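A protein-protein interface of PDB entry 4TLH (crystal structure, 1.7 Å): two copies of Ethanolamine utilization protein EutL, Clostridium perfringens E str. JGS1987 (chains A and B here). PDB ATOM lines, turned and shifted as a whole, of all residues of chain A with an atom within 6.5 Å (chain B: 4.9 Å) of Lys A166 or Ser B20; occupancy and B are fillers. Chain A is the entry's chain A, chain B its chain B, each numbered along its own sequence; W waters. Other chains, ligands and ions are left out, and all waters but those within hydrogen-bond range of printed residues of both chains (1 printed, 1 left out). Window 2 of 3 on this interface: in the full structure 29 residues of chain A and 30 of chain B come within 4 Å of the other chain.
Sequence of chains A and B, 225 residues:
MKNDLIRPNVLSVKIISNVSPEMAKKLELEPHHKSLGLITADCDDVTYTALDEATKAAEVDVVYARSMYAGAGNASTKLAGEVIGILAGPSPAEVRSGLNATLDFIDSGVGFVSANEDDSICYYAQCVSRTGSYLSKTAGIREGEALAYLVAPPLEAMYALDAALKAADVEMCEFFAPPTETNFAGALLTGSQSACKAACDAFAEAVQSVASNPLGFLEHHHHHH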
ATOM      1  N   LEU A 161      15.721 -20.778  14.401  1.00  0.00           N
ATOM      2  CA  LEU A 161      14.614 -20.616  15.331  1.00  0.00           C
ATOM      3  C   LEU A 161      14.822 -21.488  16.545  1.00  0.00           C
ATOM      4  O   LEU A 161      14.678 -21.035  17.681  1.00  0.00           O
ATOM      5  CB  LEU A 161      13.278 -20.957  14.687  1.00  0.00           C
ATOM      6  CG  LEU A 161      12.664 -19.909  13.764  1.00  0.00           C
ATOM      7  CD1 LEU A 161      11.360 -20.434  13.238  1.00  0.00           C
ATOM      8  CD2 LEU A 161      12.474 -18.581  14.472  1.00  0.00           C
ATOM      9  N   ASP A 162      15.159 -22.747  16.304  1.00  0.00           N
ATOM     10  CA  ASP A 162      15.396 -23.648  17.389  1.00  0.00           C
ATOM     11  C   ASP A 162      16.551 -23.124  18.233  1.00  0.00           C
ATOM     12  O   ASP A 162      16.510 -23.183  19.460  1.00  0.00           O
ATOM     13  CB  ASP A 162      15.675 -25.050  16.869  1.00  0.00           C
ATOM     14  CG  ASP A 162      15.853 -26.033  17.981  1.00  0.00           C
ATOM     15  OD1 ASP A 162      14.865 -26.327  18.688  1.00  0.00           O
ATOM     16  OD2 ASP A 162      16.984 -26.484  18.157  1.00  0.00           O
ATOM     17  N   ALA A 163      17.568 -22.566  17.581  1.00  0.00           N
ATOM     18  CA  ALA A 163      18.699 -21.978  18.307  1.00  0.00           C
ATOM     19  C   ALA A 163      18.270 -20.780  19.170  1.00  0.00           C
ATOM     20  O   ALA A 163      18.699 -20.631  20.315  1.00  0.00           O
ATOM     21  CB  ALA A 163      19.779 -21.557  17.331  1.00  0.00           C
ATOM     22  N   ALA A 164      17.410 -19.932  18.621  1.00  0.00           N
ATOM     23  CA  ALA A 164      16.956 -18.741  19.334  1.00  0.00           C
ATOM     24  C   ALA A 164      16.116 -19.116  20.548  1.00  0.00           C
ATOM     25  O   ALA A 164      16.188 -18.482  21.586  1.00  0.00           O
ATOM     26  CB  ALA A 164      16.170 -17.851  18.391  1.00  0.00           C
ATOM     27  N   LEU A 165      15.328 -20.174  20.423  1.00  0.00           N
ATOM     28  CA  LEU A 165      14.474 -20.604  21.519  1.00  0.00           C
ATOM     29  C   LEU A 165      15.309 -21.152  22.679  1.00  0.00           C
ATOM     30  O   LEU A 165      14.950 -20.975  23.838  1.00  0.00           O
ATOM     31  CB  LEU A 165      13.465 -21.637  21.003  1.00  0.00           C
ATOM     32  CG  LEU A 165      12.351 -20.989  20.168  1.00  0.00           C
ATOM     33  CD1 LEU A 165      11.662 -22.037  19.265  1.00  0.00           C
ATOM     34  CD2 LEU A 165      11.340 -20.283  21.060  1.00  0.00           C
ATOM     35  N   LYS A 166      16.430 -21.798  22.366  1.00  0.00           N
ATOM     36  CA  LYS A 166      17.353 -22.297  23.393  1.00  0.00           C
ATOM     37  C   LYS A 166      18.173 -21.190  24.031  1.00  0.00           C
ATOM     38  O   LYS A 166      18.621 -21.320  25.166  1.00  0.00           O
ATOM     39  CB  LYS A 166      18.320 -23.321  22.806  1.00  0.00           C
ATOM     40  CG  LYS A 166      17.701 -24.594  22.386  1.00  0.00           C
ATOM     41  CD  LYS A 166      18.768 -25.542  21.907  1.00  0.00           C
ATOM     42  CE  LYS A 166      18.373 -26.158  20.604  1.00  0.00           C
ATOM     43  NZ  LYS A 166      19.303 -27.232  20.202  1.00  0.00           N
ATOM     44  N   ALA A 167      18.402 -20.122  23.277  1.00  0.00           N
ATOM     45  CA  ALA A 167      19.323 -19.065  23.695  1.00  0.00           C
ATOM     46  C   ALA A 167      18.690 -18.032  24.628  1.00  0.00           C
ATOM     47  O   ALA A 167      19.391 -17.401  25.421  1.00  0.00           O
ATOM     48  CB  ALA A 167      19.888 -18.364  22.463  1.00  0.00           C
ATOM     49  N   ALA A 168      17.370 -17.866  24.547  1.00  0.00           N
ATOM     50  CA  ALA A 168      16.710 -16.768  25.239  1.00  0.00           C
ATOM     51  C   ALA A 168      15.414 -17.204  25.934  1.00  0.00           C
ATOM     52  O   ALA A 168      14.817 -18.226  25.579  1.00  0.00           O
ATOM     53  CB  ALA A 168      16.432 -15.642  24.242  1.00  0.00           C
ATOM     54  N   ASP A 169      14.998 -16.431  26.934  1.00  0.00           N
ATOM     55  CA  ASP A 169      13.754 -16.710  27.642  1.00  0.00           C
ATOM     56  C   ASP A 169      12.567 -16.125  26.862  1.00  0.00           C
ATOM     57  O   ASP A 169      11.936 -15.155  27.276  1.00  0.00           O
ATOM     58  CB  ASP A 169      13.805 -16.147  29.068  1.00  0.00           C
ATOM     59  CG  ASP A 169      12.717 -16.718  29.964  1.00  0.00           C
ATOM     60  OD1 ASP A 169      12.161 -17.788  29.633  1.00  0.00           O
ATOM     61  OD2 ASP A 169      12.425 -16.099  31.013  1.00  0.00           O
ATOM     62  N   VAL A 170      12.283 -16.729  25.726  1.00  0.00           N
ATOM     63  CA  VAL A 170      11.191 -16.263  24.855  1.00  0.00           C
ATOM     64  C   VAL A 170      10.218 -17.408  24.639  1.00  0.00           C
ATOM     65  O   VAL A 170      10.563 -18.558  24.888  1.00  0.00           O
ATOM     66  CB  VAL A 170      11.727 -15.742  23.518  1.00  0.00           C
ATOM     67  CG1 VAL A 170      12.424 -14.390  23.727  1.00  0.00           C
ATOM     68  CG2 VAL A 170      12.671 -16.760  22.896  1.00  0.00           C
ATOM     69  N   ILE B  16      20.539 -31.044  14.260  1.00  0.00           N
ATOM     70  CA  ILE B  16      20.274 -30.406  15.541  1.00  0.00           C
ATOM     71  C   ILE B  16      20.270 -31.479  16.608  1.00  0.00           C
ATOM     72  O   ILE B  16      19.487 -32.429  16.516  1.00  0.00           O
ATOM     73  CB  ILE B  16      18.905 -29.691  15.565  1.00  0.00           C
ATOM     74  CG1 ILE B  16      18.855 -28.593  14.511  1.00  0.00           C
ATOM     75  CG2 ILE B  16      18.615 -29.128  16.970  1.00  0.00           C
ATOM     76  CD1 ILE B  16      17.471 -28.003  14.312  1.00  0.00           C
ATOM     77  N   SER B  17      21.062 -31.245  17.655  1.00  0.00           N
ATOM     78  CA  SER B  17      20.987 -32.006  18.904  1.00  0.00           C
ATOM     79  C   SER B  17      20.032 -31.322  19.882  1.00  0.00           C
ATOM     80  O   SER B  17      19.999 -30.097  19.962  1.00  0.00           O
ATOM     81  CB  SER B  17      22.367 -32.125  19.577  1.00  0.00           C
ATOM     82  OG  SER B  17      23.316 -32.784  18.759  1.00  0.00           O
ATOM     83  N   ASN B  18      19.295 -32.123  20.649  1.00  0.00           N
ATOM     84  CA  ASN B  18      18.515 -31.626  21.781  1.00  0.00           C
ATOM     85  C   ASN B  18      17.587 -30.477  21.383  1.00  0.00           C
ATOM     86  O   ASN B  18      17.668 -29.367  21.919  1.00  0.00           O
ATOM     87  CB  ASN B  18      19.456 -31.195  22.908  1.00  0.00           C
ATOM     88  CG  ASN B  18      20.298 -32.347  23.442  1.00  0.00           C
ATOM     89  OD1 ASN B  18      19.792 -33.444  23.693  1.00  0.00           O
ATOM     90  ND2 ASN B  18      21.594 -32.104  23.604  1.00  0.00           N
ATOM     91  N   VAL B  19      16.717 -30.765  20.422  1.00  0.00           N
ATOM     92  CA  VAL B  19      15.731 -29.812  19.922  1.00  0.00           C
ATOM     93  C   VAL B  19      14.960 -29.141  21.063  1.00  0.00           C
ATOM     94  O   VAL B  19      14.629 -29.772  22.070  1.00  0.00           O
ATOM     95  CB  VAL B  19      14.754 -30.526  18.949  1.00  0.00           C
ATOM     96  CG1 VAL B  19      14.018 -31.643  19.659  1.00  0.00           C
ATOM     97  CG2 VAL B  19      13.784 -29.543  18.324  1.00  0.00           C
ATOM     98  N   SER B  20      14.694 -27.849  20.915  1.00  0.00           N
ATOM     99  CA  SER B  20      14.036 -27.097  21.962  1.00  0.00           C
ATOM    100  C   SER B  20      12.629 -27.643  22.217  1.00  0.00           C
ATOM    101  O   SER B  20      11.950 -28.076  21.285  1.00  0.00           O
ATOM    102  CB  SER B  20      13.957 -25.621  21.582  1.00  0.00           C
ATOM    103  OG  SER B  20      13.193 -25.475  20.400  1.00  0.00           O
ATOM    104  N   PRO B  21      12.188 -27.625  23.483  1.00  0.00           N
ATOM    105  CA  PRO B  21      10.805 -28.006  23.788  1.00  0.00           C
ATOM    106  C   PRO B  21       9.765 -27.268  22.941  1.00  0.00           C
ATOM    107  O   PRO B  21       8.744 -27.838  22.572  1.00  0.00           O
ATOM    108  CB  PRO B  21      10.653 -27.619  25.249  1.00  0.00           C
ATOM    109  CG  PRO B  21      12.026 -27.675  25.805  1.00  0.00           C
ATOM    110  CD  PRO B  21      12.948 -27.273  24.695  1.00  0.00           C
ATOM    111  N   GLU B  22      10.028 -25.996  22.667  1.00  0.00           N
ATOM    112  CA  GLU B  22       9.089 -25.157  21.948  1.00  0.00           C
ATOM    113  C   GLU B  22       8.969 -25.619  20.506  1.00  0.00           C
ATOM    114  O   GLU B  22       7.866 -25.773  19.983  1.00  0.00           O
ATOM    115  CB  GLU B  22       9.521 -23.684  22.027  1.00  0.00           C
ATOM    116  CG  GLU B  22       9.485 -23.091  23.450  1.00  0.00           C
ATOM    117  CD  GLU B  22      10.808 -23.212  24.216  1.00  0.00           C
ATOM    118  OE1 GLU B  22      11.655 -24.070  23.873  1.00  0.00           O
ATOM    119  OE2 GLU B  22      11.003 -22.426  25.176  1.00  0.00           O
ATOM    120  N   MET B  23      10.101 -25.886  19.870  1.00  0.00           N
ATOM    121  CA  MET B  23      10.100 -26.388  18.511  1.00  0.00           C
ATOM    122  C   MET B  23       9.503 -27.795  18.455  1.00  0.00           C
ATOM    123  O   MET B  23       8.774 -28.121  17.532  1.00  0.00           O
ATOM    124  CB  MET B  23      11.520 -26.382  17.940  1.00  0.00           C
ATOM    125  CG  MET B  23      11.617 -26.613  16.452  1.00  0.00           C
ATOM    126  SD  MET B  23      10.666 -25.414  15.466  1.00  0.00           S
ATOM    127  CE  MET B  23      10.964 -23.896  16.361  1.00  0.00           C
ATOM    128  N   ALA B  24       9.803 -28.627  19.446  1.00  0.00           N
ATOM    129  CA  ALA B  24       9.254 -29.984  19.490  1.00  0.00           C
ATOM    130  C   ALA B  24       7.731 -29.950  19.538  1.00  0.00           C
ATOM    131  O   ALA B  24       7.051 -30.725  18.867  1.00  0.00           O
ATOM    132  CB  ALA B  24       9.811 -30.743  20.707  1.00  0.00           C
HETATM  133  O   HOH W   1      14.163 -23.750  24.967  1.00  0.00           O
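Among the printed residues, pairs that only touch across the chains: Asp A162 with Ile B16, Asp A162 with Val B19, Asp A162 with Met B23, Leu A165 with Ser B20, Leu A165 with Glu B22, Leu A165 with Met B23, Lys A166 with Ile B16, Lys A166 with Ser B20 and Val A170 with Glu B22.
No position is printed for both chains.
Of the 12 pairs that touch across the chains among the printed residues, none has its exchanged pair printed and touching as well.
Water W1 bridges OE1 of Glu B22 (2.8 Å) and O of Leu A165 (3.1 Å).
Printed residues of chain B within 4 Å of Lys A166: Ile B16 (3.8 Å), Ser B17 (3.0 Å), Asn B18 (3.2 Å) and Ser B20 (3.96 Å).
Ser B20 touches three residues of chain A.
Printed residues of chain B within 4 Å of Leu A165: Ser B20, Glu B22 and Met B23.
Of the printed residues of chain B, Asp A162 touches Ile B16, Val B19, Ser B20 and Met B23.
Printed residues of chain A within 4 Å of Ile B16: Asp A162 (3.3 Å) and Lys A166 (3.8 Å).
Leu A161 touches none of the printed residues of chain B.
Pro B21 touches none of the printed residues of chain A.
OD1 of Asp A162 sits at hydrogen-bond distance from OG of Ser B20, 2.5 Å away.
NZ of Lys A166 is in hydrogen-bond range of O of Ser B17, 3.0 Å away.
The side-chain amino group (NZ) of Lys A166 is in hydrogen-bond range of the backbone carbonyl oxygen (O) of Asn B18 (3.2 Å).
The side-chain hydroxyl (OG) of Ser B20 lies close to the backbone NH (N) of Met B23, 3.2 Å away.
The side-chain carboxylate (OD2) of Asp A162 lies within salt-bridge range of the side-chain amino group (NZ) of Lys A166 (3.2 Å).
Printed residues of chain A that touch a printed residue of chain B: Asp A162, Leu A165, Lys A166 and Val A170.
Hydrophobic or aromatic side chains of chain A that line the printed part of chain B: Leu A165.
Printed residues of chain B that touch a printed residue of chain A: Ile B16, Ser B17, Asn B18, Val B19, Ser B20, Glu B22 and Met B23.
Among the printed residues, 12 pairs touch across the chains.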
